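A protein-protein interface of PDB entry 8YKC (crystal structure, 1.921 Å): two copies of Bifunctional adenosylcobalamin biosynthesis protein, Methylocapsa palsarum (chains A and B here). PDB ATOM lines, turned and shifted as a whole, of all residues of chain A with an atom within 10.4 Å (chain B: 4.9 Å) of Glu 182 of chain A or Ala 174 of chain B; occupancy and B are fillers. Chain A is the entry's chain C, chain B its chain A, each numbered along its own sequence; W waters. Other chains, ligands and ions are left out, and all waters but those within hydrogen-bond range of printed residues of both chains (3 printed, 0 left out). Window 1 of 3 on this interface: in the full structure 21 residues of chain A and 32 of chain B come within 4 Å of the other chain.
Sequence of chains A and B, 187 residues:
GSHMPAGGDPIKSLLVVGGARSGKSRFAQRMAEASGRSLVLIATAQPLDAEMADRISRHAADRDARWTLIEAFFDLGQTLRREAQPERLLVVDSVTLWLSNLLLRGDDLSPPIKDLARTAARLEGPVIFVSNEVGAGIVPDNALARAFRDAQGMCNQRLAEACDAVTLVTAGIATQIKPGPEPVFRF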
ATOM      1  N   GLN A 157      26.139  21.536  20.193  1.00  0.00           N
ATOM      2  CA  GLN A 157      25.295  21.656  21.416  1.00  0.00           C
ATOM      3  C   GLN A 157      24.804  23.118  21.550  1.00  0.00           C
ATOM      4  O   GLN A 157      23.608  23.325  21.875  1.00  0.00           O
ATOM      5  CB  GLN A 157      26.077  21.252  22.659  1.00  0.00           C
ATOM      6  CG  GLN A 157      26.318  19.765  22.820  1.00  0.00           C
ATOM      7  CD  GLN A 157      27.156  19.567  24.060  1.00  0.00           C
ATOM      8  OE1 GLN A 157      26.755  19.859  25.178  1.00  0.00           O
ATOM      9  NE2 GLN A 157      28.383  19.153  23.865  1.00  0.00           N
ATOM     10  N   ALA A 160      22.304  23.992  18.772  1.00  0.00           N
ATOM     11  CA  ALA A 160      21.043  23.271  19.045  1.00  0.00           C
ATOM     12  C   ALA A 160      20.229  24.030  20.101  1.00  0.00           C
ATOM     13  O   ALA A 160      19.018  24.063  19.952  1.00  0.00           O
ATOM     14  CB  ALA A 160      21.292  21.863  19.492  1.00  0.00           C
ATOM     15  N   GLU A 161      20.866  24.518  21.158  1.00  0.00           N
ATOM     16  CA  GLU A 161      20.217  25.201  22.308  1.00  0.00           C
ATOM     17  C   GLU A 161      19.651  26.530  21.796  1.00  0.00           C
ATOM     18  O   GLU A 161      18.540  26.830  22.136  1.00  0.00           O
ATOM     19  CB  GLU A 161      21.206  25.341  23.462  1.00  0.00           C
ATOM     20  CG  GLU A 161      20.712  26.122  24.679  1.00  0.00           C
ATOM     21  CD  GLU A 161      21.770  26.247  25.774  1.00  0.00           C
ATOM     22  OE1 GLU A 161      21.488  25.824  26.934  1.00  0.00           O
ATOM     23  OE2 GLU A 161      22.921  26.704  25.464  1.00  0.00           O
ATOM     24  N   ALA A 162      20.395  27.281  20.993  1.00  0.00           N
ATOM     25  CA  ALA A 162      19.983  28.633  20.517  1.00  0.00           C
ATOM     26  C   ALA A 162      18.885  28.552  19.438  1.00  0.00           C
ATOM     27  O   ALA A 162      18.067  29.488  19.332  1.00  0.00           O
ATOM     28  CB  ALA A 162      21.185  29.374  19.996  1.00  0.00           C
ATOM     29  N   CYS A 163      18.894  27.526  18.597  1.00  0.00           N
ATOM     30  CA  CYS A 163      18.006  27.440  17.404  1.00  0.00           C
ATOM     31  C   CYS A 163      16.597  26.990  17.841  1.00  0.00           C
ATOM     32  O   CYS A 163      16.456  26.209  18.800  1.00  0.00           O
ATOM     33  CB  CYS A 163      18.576  26.524  16.314  1.00  0.00           C
ATOM     34  SG  CYS A 163      20.024  27.191  15.445  1.00  0.00           S
ATOM     35  N   ASP A 164      15.576  27.447  17.125  1.00  0.00           N
ATOM     36  CA  ASP A 164      14.159  27.058  17.352  1.00  0.00           C
ATOM     37  C   ASP A 164      13.931  25.590  17.013  1.00  0.00           C
ATOM     38  O   ASP A 164      13.141  24.953  17.703  1.00  0.00           O
ATOM     39  CB  ASP A 164      13.212  27.925  16.527  1.00  0.00           C
ATOM     40  CG  ASP A 164      13.252  29.389  16.928  1.00  0.00           C
ATOM     41  OD1 ASP A 164      13.588  29.667  18.090  1.00  0.00           O
ATOM     42  OD2 ASP A 164      13.016  30.249  16.043  1.00  0.00           O
ATOM     43  N   VAL A 166      15.752  21.737  15.255  1.00  0.00           N
ATOM     44  CA  VAL A 166      16.948  20.885  15.028  1.00  0.00           C
ATOM     45  C   VAL A 166      16.408  19.618  14.386  1.00  0.00           C
ATOM     46  O   VAL A 166      15.425  19.074  14.917  1.00  0.00           O
ATOM     47  CB  VAL A 166      17.699  20.581  16.346  1.00  0.00           C
ATOM     48  CG1 VAL A 166      18.943  19.751  16.091  1.00  0.00           C
ATOM     49  CG2 VAL A 166      18.029  21.827  17.123  1.00  0.00           C
ATOM     50  N   LEU A 168      17.916  15.869  12.579  1.00  0.00           N
ATOM     51  CA  LEU A 168      19.019  14.929  12.287  1.00  0.00           C
ATOM     52  C   LEU A 168      18.724  14.345  10.919  1.00  0.00           C
ATOM     53  O   LEU A 168      17.562  13.900  10.713  1.00  0.00           O
ATOM     54  CB  LEU A 168      19.075  13.822  13.342  1.00  0.00           C
ATOM     55  CG  LEU A 168      19.400  14.268  14.760  1.00  0.00           C
ATOM     56  CD1 LEU A 168      19.623  13.049  15.631  1.00  0.00           C
ATOM     57  CD2 LEU A 168      20.610  15.202  14.825  1.00  0.00           C
ATOM     58  N   THR A 175      14.832  13.752  10.493  1.00  0.00           N
ATOM     59  CA  THR A 175      14.037  13.509  11.717  1.00  0.00           C
ATOM     60  C   THR A 175      14.129  14.750  12.621  1.00  0.00           C
ATOM     61  O   THR A 175      15.238  15.162  12.949  1.00  0.00           O
ATOM     62  CB  THR A 175      14.508  12.242  12.437  1.00  0.00           C
ATOM     63  OG1 THR A 175      14.464  11.162  11.502  1.00  0.00           O
ATOM     64  CG2 THR A 175      13.658  11.910  13.645  1.00  0.00           C
ATOM     65  N   GLN A 176      12.992  15.316  13.013  1.00  0.00           N
ATOM     66  CA  GLN A 176      12.946  16.493  13.916  1.00  0.00           C
ATOM     67  C   GLN A 176      13.215  16.024  15.342  1.00  0.00           C
ATOM     68  O   GLN A 176      12.541  15.099  15.767  1.00  0.00           O
ATOM     69  CB  GLN A 176      11.587  17.187  13.837  1.00  0.00           C
ATOM     70  CG  GLN A 176      11.512  18.453  14.676  1.00  0.00           C
ATOM     71  CD  GLN A 176      10.187  19.160  14.499  1.00  0.00           C
ATOM     72  OE1 GLN A 176       9.466  19.416  15.462  1.00  0.00           O
ATOM     73  NE2 GLN A 176       9.866  19.480  13.258  1.00  0.00           N
ATOM     74  N   ILE A 177      14.142  16.670  16.053  1.00  0.00           N
ATOM     75  CA  ILE A 177      14.376  16.396  17.498  1.00  0.00           C
ATOM     76  C   ILE A 177      14.051  17.638  18.325  1.00  0.00           C
ATOM     77  O   ILE A 177      13.987  17.527  19.587  1.00  0.00           O
ATOM     78  CB  ILE A 177      15.808  15.879  17.735  1.00  0.00           C
ATOM     79  CG1 ILE A 177      16.861  16.915  17.339  1.00  0.00           C
ATOM     80  CG2 ILE A 177      16.009  14.565  17.009  1.00  0.00           C
ATOM     81  CD1 ILE A 177      18.254  16.555  17.772  1.00  0.00           C
ATOM     82  N   LYS A 178      13.898  18.788  17.676  1.00  0.00           N
ATOM     83  CA  LYS A 178      13.487  20.048  18.338  1.00  0.00           C
ATOM     84  C   LYS A 178      12.711  20.877  17.315  1.00  0.00           C
ATOM     85  O   LYS A 178      13.046  20.900  16.130  1.00  0.00           O
ATOM     86  CB  LYS A 178      14.687  20.767  18.968  1.00  0.00           C
ATOM     87  CG  LYS A 178      14.357  22.096  19.660  1.00  0.00           C
ATOM     88  CD  LYS A 178      15.579  22.950  19.995  1.00  0.00           C
ATOM     89  CE  LYS A 178      15.277  24.161  20.870  1.00  0.00           C
ATOM     90  NZ  LYS A 178      16.449  25.050  21.032  1.00  0.00           N
ATOM     91  N   PRO A 179      11.552  21.470  17.679  1.00  0.00           N
ATOM     92  CA  PRO A 179      10.962  21.345  19.011  1.00  0.00           C
ATOM     93  C   PRO A 179      10.327  19.963  19.265  1.00  0.00           C
ATOM     94  O   PRO A 179      10.139  19.165  18.343  1.00  0.00           O
ATOM     95  CB  PRO A 179       9.938  22.500  19.051  1.00  0.00           C
ATOM     96  CG  PRO A 179       9.573  22.765  17.616  1.00  0.00           C
ATOM     97  CD  PRO A 179      10.753  22.306  16.769  1.00  0.00           C
ATOM     98  N   GLY A 180      10.044  19.698  20.540  1.00  0.00           N
ATOM     99  CA  GLY A 180       9.624  18.389  21.060  1.00  0.00           C
ATOM    100  C   GLY A 180      10.099  18.243  22.501  1.00  0.00           C
ATOM    101  O   GLY A 180      11.233  18.589  22.808  1.00  0.00           O
ATOM    102  N   PRO A 181       9.252  17.812  23.452  1.00  0.00           N
ATOM    103  CA  PRO A 181       9.696  17.676  24.840  1.00  0.00           C
ATOM    104  C   PRO A 181      10.831  16.647  24.920  1.00  0.00           C
ATOM    105  O   PRO A 181      10.747  15.635  24.284  1.00  0.00           O
ATOM    106  CB  PRO A 181       8.436  17.225  25.587  1.00  0.00           C
ATOM    107  CG  PRO A 181       7.318  17.671  24.689  1.00  0.00           C
ATOM    108  CD  PRO A 181       7.840  17.442  23.282  1.00  0.00           C
ATOM    109  N   GLU A 182      11.916  17.001  25.598  1.00  0.00           N
ATOM    110  CA  GLU A 182      13.012  16.063  25.916  1.00  0.00           C
ATOM    111  C   GLU A 182      12.473  15.100  26.961  1.00  0.00           C
ATOM    112  O   GLU A 182      11.601  15.480  27.739  1.00  0.00           O
ATOM    113  CB  GLU A 182      14.269  16.832  26.320  1.00  0.00           C
ATOM    114  CG  GLU A 182      14.894  17.506  25.107  1.00  0.00           C
ATOM    115  CD  GLU A 182      16.306  17.992  25.309  1.00  0.00           C
ATOM    116  OE1 GLU A 182      16.545  19.199  25.085  1.00  0.00           O
ATOM    117  OE2 GLU A 182      17.150  17.170  25.718  1.00  0.00           O
ATOM    118  N   PRO A 183      12.895  13.815  26.921  1.00  0.00           N
ATOM    119  CA  PRO A 183      12.401  12.806  27.853  1.00  0.00           C
ATOM    120  C   PRO A 183      12.919  13.154  29.249  1.00  0.00           C
ATOM    121  O   PRO A 183      13.922  13.863  29.361  1.00  0.00           O
ATOM    122  CB  PRO A 183      12.968  11.486  27.300  1.00  0.00           C
ATOM    123  CG  PRO A 183      14.226  11.920  26.600  1.00  0.00           C
ATOM    124  CD  PRO A 183      13.885  13.259  25.981  1.00  0.00           C
ATOM    125  N   VAL A 184      12.176  12.696  30.255  1.00  0.00           N
ATOM    126  CA  VAL A 184      12.457  12.843  31.701  1.00  0.00           C
ATOM    127  C   VAL A 184      12.321  11.442  32.302  1.00  0.00           C
ATOM    128  O   VAL A 184      11.447  10.671  31.872  1.00  0.00           O
ATOM    129  CB  VAL A 184      11.535  13.907  32.335  1.00  0.00           C
ATOM    130  CG1 VAL A 184      11.600  13.896  33.859  1.00  0.00           C
ATOM    131  CG2 VAL A 184      11.883  15.279  31.793  1.00  0.00           C
ATOM    132  N   PHE A 185      13.267  11.089  33.158  1.00  0.00           N
ATOM    133  CA  PHE A 185      13.325   9.789  33.871  1.00  0.00           C
ATOM    134  C   PHE A 185      13.366  10.088  35.368  1.00  0.00           C
ATOM    135  O   PHE A 185      14.068  11.014  35.765  1.00  0.00           O
ATOM    136  CB  PHE A 185      14.545   9.003  33.402  1.00  0.00           C
ATOM    137  CG  PHE A 185      14.496   8.732  31.932  1.00  0.00           C
ATOM    138  CD1 PHE A 185      13.562   7.856  31.426  1.00  0.00           C
ATOM    139  CD2 PHE A 185      15.293   9.452  31.061  1.00  0.00           C
ATOM    140  CE1 PHE A 185      13.495   7.627  30.062  1.00  0.00           C
ATOM    141  CE2 PHE A 185      15.218   9.227  29.699  1.00  0.00           C
ATOM    142  CZ  PHE A 185      14.313   8.319  29.204  1.00  0.00           C
ATOM    143  N   PHE B  27      23.235  15.613  30.363  1.00  0.00           N
ATOM    144  CA  PHE B  27      21.873  15.018  30.388  1.00  0.00           C
ATOM    145  C   PHE B  27      21.749  14.158  31.646  1.00  0.00           C
ATOM    146  O   PHE B  27      20.775  14.309  32.408  1.00  0.00           O
ATOM    147  CB  PHE B  27      21.547  14.182  29.149  1.00  0.00           C
ATOM    148  CG  PHE B  27      20.156  13.611  29.220  1.00  0.00           C
ATOM    149  CD1 PHE B  27      19.058  14.425  29.011  1.00  0.00           C
ATOM    150  CD2 PHE B  27      19.942  12.292  29.587  1.00  0.00           C
ATOM    151  CE1 PHE B  27      17.768  13.931  29.123  1.00  0.00           C
ATOM    152  CE2 PHE B  27      18.649  11.802  29.713  1.00  0.00           C
ATOM    153  CZ  PHE B  27      17.565  12.627  29.492  1.00  0.00           C
ATOM    154  N   ARG B  30      21.598  16.191  34.796  1.00  0.00           N
ATOM    155  CA  ARG B  30      20.295  16.910  34.940  1.00  0.00           C
ATOM    156  C   ARG B  30      19.274  15.928  35.501  1.00  0.00           C
ATOM    157  O   ARG B  30      18.570  16.291  36.485  1.00  0.00           O
ATOM    158  CB  ARG B  30      19.788  17.457  33.599  1.00  0.00           C
ATOM    159  CG  ARG B  30      20.074  18.921  33.311  1.00  0.00           C
ATOM    160  CD  ARG B  30      20.017  19.208  31.815  1.00  0.00           C
ATOM    161  NE  ARG B  30      18.913  18.610  31.063  1.00  0.00           N
ATOM    162  CZ  ARG B  30      19.000  18.250  29.773  1.00  0.00           C
ATOM    163  NH1 ARG B  30      20.162  18.400  29.146  1.00  0.00           N
ATOM    164  NH2 ARG B  30      17.957  17.723  29.122  1.00  0.00           N
ATOM    165  N   THR B 167      18.472   6.404  26.294  1.00  0.00           N
ATOM    166  CA  THR B 167      18.341   7.671  25.565  1.00  0.00           C
ATOM    167  C   THR B 167      19.594   7.864  24.710  1.00  0.00           C
ATOM    168  O   THR B 167      20.719   7.483  25.169  1.00  0.00           O
ATOM    169  CB  THR B 167      17.986   8.785  26.552  1.00  0.00           C
ATOM    170  OG1 THR B 167      17.723   9.968  25.794  1.00  0.00           O
ATOM    171  CG2 THR B 167      19.079   9.004  27.560  1.00  0.00           C
ATOM    172  N   LEU B 168      19.379   8.427  23.530  1.00  0.00           N
ATOM    173  CA  LEU B 168      20.423   8.877  22.604  1.00  0.00           C
ATOM    174  C   LEU B 168      20.535  10.379  22.746  1.00  0.00           C
ATOM    175  O   LEU B 168      19.513  11.075  22.614  1.00  0.00           O
ATOM    176  CB  LEU B 168      20.038   8.549  21.169  1.00  0.00           C
ATOM    177  CG  LEU B 168      19.872   7.089  20.837  1.00  0.00           C
ATOM    178  CD1 LEU B 168      19.712   6.949  19.335  1.00  0.00           C
ATOM    179  CD2 LEU B 168      21.028   6.246  21.368  1.00  0.00           C
ATOM    180  N   VAL B 169      21.727  10.885  22.995  1.00  0.00           N
ATOM    181  CA  VAL B 169      21.879  12.352  23.085  1.00  0.00           C
ATOM    182  C   VAL B 169      22.683  12.813  21.877  1.00  0.00           C
ATOM    183  O   VAL B 169      23.774  12.252  21.644  1.00  0.00           O
ATOM    184  CB  VAL B 169      22.516  12.723  24.438  1.00  0.00           C
ATOM    185  CG1 VAL B 169      22.769  14.213  24.551  1.00  0.00           C
ATOM    186  CG2 VAL B 169      21.657  12.226  25.601  1.00  0.00           C
ATOM    187  N   GLY B 172      23.407  17.767  22.181  1.00  0.00           N
ATOM    188  CA  GLY B 172      22.913  18.175  23.506  1.00  0.00           C
ATOM    189  C   GLY B 172      21.424  17.895  23.721  1.00  0.00           C
ATOM    190  O   GLY B 172      20.923  18.276  24.780  1.00  0.00           O
ATOM    191  N   ILE B 173      20.738  17.263  22.764  1.00  0.00           N
ATOM    192  CA  ILE B 173      19.288  16.959  22.831  1.00  0.00           C
ATOM    193  C   ILE B 173      19.070  15.451  22.973  1.00  0.00           C
ATOM    194  O   ILE B 173      19.606  14.643  22.112  1.00  0.00           O
ATOM    195  CB  ILE B 173      18.594  17.553  21.589  1.00  0.00           C
ATOM    196  CG1 ILE B 173      18.777  19.072  21.529  1.00  0.00           C
ATOM    197  CG2 ILE B 173      17.137  17.125  21.516  1.00  0.00           C
ATOM    198  CD1 ILE B 173      18.327  19.653  20.217  1.00  0.00           C
ATOM    199  N   ALA B 174      18.355  15.051  24.030  1.00  0.00           N
ATOM    200  CA  ALA B 174      18.020  13.647  24.337  1.00  0.00           C
ATOM    201  C   ALA B 174      16.795  13.199  23.541  1.00  0.00           C
ATOM    202  O   ALA B 174      15.798  13.952  23.416  1.00  0.00           O
ATOM    203  CB  ALA B 174      17.785  13.466  25.830  1.00  0.00           C
ATOM    204  N   THR B 175      16.872  11.999  23.007  1.00  0.00           N
ATOM    205  CA  THR B 175      15.714  11.264  22.432  1.00  0.00           C
ATOM    206  C   THR B 175      15.624   9.906  23.117  1.00  0.00           C
ATOM    207  O   THR B 175      16.623   9.152  23.090  1.00  0.00           O
ATOM    208  CB  THR B 175      15.837  11.052  20.915  1.00  0.00           C
ATOM    209  OG1 THR B 175      16.033  12.315  20.291  1.00  0.00           O
ATOM    210  CG2 THR B 175      14.637  10.342  20.327  1.00  0.00           C
ATOM    211  N   GLN B 176      14.427   9.573  23.618  1.00  0.00           N
ATOM    212  CA  GLN B 176      14.141   8.269  24.251  1.00  0.00           C
ATOM    213  C   GLN B 176      14.038   7.212  23.157  1.00  0.00           C
ATOM    214  O   GLN B 176      13.302   7.468  22.190  1.00  0.00           O
ATOM    215  CB  GLN B 176      12.817   8.336  25.014  1.00  0.00           C
ATOM    216  CG  GLN B 176      12.452   7.004  25.694  1.00  0.00           C
ATOM    217  CD  GLN B 176      11.291   7.103  26.647  1.00  0.00           C
ATOM    218  OE1 GLN B 176      10.458   6.192  26.756  1.00  0.00           O
ATOM    219  NE2 GLN B 176      11.246   8.204  27.361  1.00  0.00           N
HETATM  220  O   HOH W   1      14.823  16.377  29.787  1.00  0.00           O
HETATM  221  O   HOH W   2      19.041  20.020  25.682  1.00  0.00           O
HETATM  222  O   HOH W   3      10.299   9.112  29.857  1.00  0.00           O
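Of the 19 printed residues of chain A, 7 touch a printed residue of chain B.
Printed residues of chain A that touch a printed residue of chain B: Gln 157, Ala 160, Val 166, Ile 177, Glu 182, Pro 183 and Phe 185.
Of the 10 printed residues of chain B, 7 touch a printed residue of chain A.
Among the printed residues, 12 pairs touch across the chains.
Positions printed for both chains: 168, 175 and 176.
Of the 12 pairs that touch across the chains among the printed residues, none has its exchanged pair printed and touching as well.
OG1 of Thr 167 of chain B is in hydrogen-bond range of O of Thr 175 of chain B (3.0 Å).
The backbone carbonyl oxygen (O) of Leu 168 of chain B is in hydrogen-bond range of the backbone NH (N) of Thr 175 of chain B, 2.8 Å away.
The backbone carbonyl oxygen of Ala 160 of chain A lies within hydrogen-bond range of the side-chain amino group of Lys 178 of chain A.
N of Ile 177 of chain A sits at hydrogen-bond distance from O of Val 166 of chain A (3.0 Å).
N of Val 166 of chain A is in hydrogen-bond range of O of Lys 178 of chain A, 3.0 Å away.
Among the printed residues, merely in contact across the chains: Pro 183 of chain A with Ala 174 of chain B (3.3 Å), Phe 185 of chain A with Gln 176 of chain B (3.6 Å), Gln 157 of chain A with Gly 172 of chain B (3.6 Å), Glu 182 of chain A with Ile 173 of chain B (3.6 Å), Pro 183 of chain A with Gln 176 of chain B (3.7 Å), Ile 177 of chain A with Ile 173 of chain B (3.7 Å), Ala 160 of chain A with Ile 173 of chain B (3.8 Å), Val 166 of chain A with Ile 173 of chain B (3.8 Å), Pro 183 of chain A with Phe 27 of chain B (3.8 Å) and Ile 177 of chain A with Thr 175 of chain B (3.98 Å).
Glu 182 of chain A touches just these residues of chain B: Arg 30, Ile 173 and Ala 174.
Ala 174 of chain B touches just these residues of chain A: Glu 182 and Pro 183.
Gly 172 of chain B touches just one residue of chain A: Gln 157.
Of chain A, only Ile 177 comes within 4 Å of Thr 175 of chain B.
Of the printed residues of chain B, Pro 183 of chain A touches Phe 27 (3.8 Å), Ala 174 (3.3 Å) and Gln 176 (3.7 Å).
Printed residues of chain A within 4 Å of Ile 173 of chain B: Ala 160, Val 166, Ile 177 and Glu 182.
Printed residues of chain B within 4 Å of Gln 157 of chain A: Gly 172.
Pro 179 of chain A touches none of the printed residues of chain B.
The nearest residue of chain B that does not touch Glu 182 of chain A is Gly 172 of chain B (4.04 Å).
The nearest residue of chain A that does not touch Ala 174 of chain B is Pro 181 of chain A (5.4 Å).
Water W2 bridges the side-chain carboxylate (OE1) of Glu 182 of chain A (2.7 Å) and the backbone carbonyl oxygen (O) of Gly 172 of chain B (2.7 Å).
Water W1 lies within hydrogen-bond range of the backbone carbonyl oxygen of Pro 183 of chain A (2.7 Å) and the guanidinium group of Arg 30 of chain B (3.5 Å).
Water W3 lies within hydrogen-bond range of O of Val 184 of chain A (2.8 Å) and NE2 of Gln 176 of chain B (2.8 Å).
OE2 of Glu 182 of chain A is in salt-bridge range of NH2 of Arg 30 of chain B (3.5 Å).
The backbone NH (N) of Ala 174 of chain B lies within hydrogen-bond range of the side-chain carboxylate (OE2) of Glu 182 of chain A (3.0 Å).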
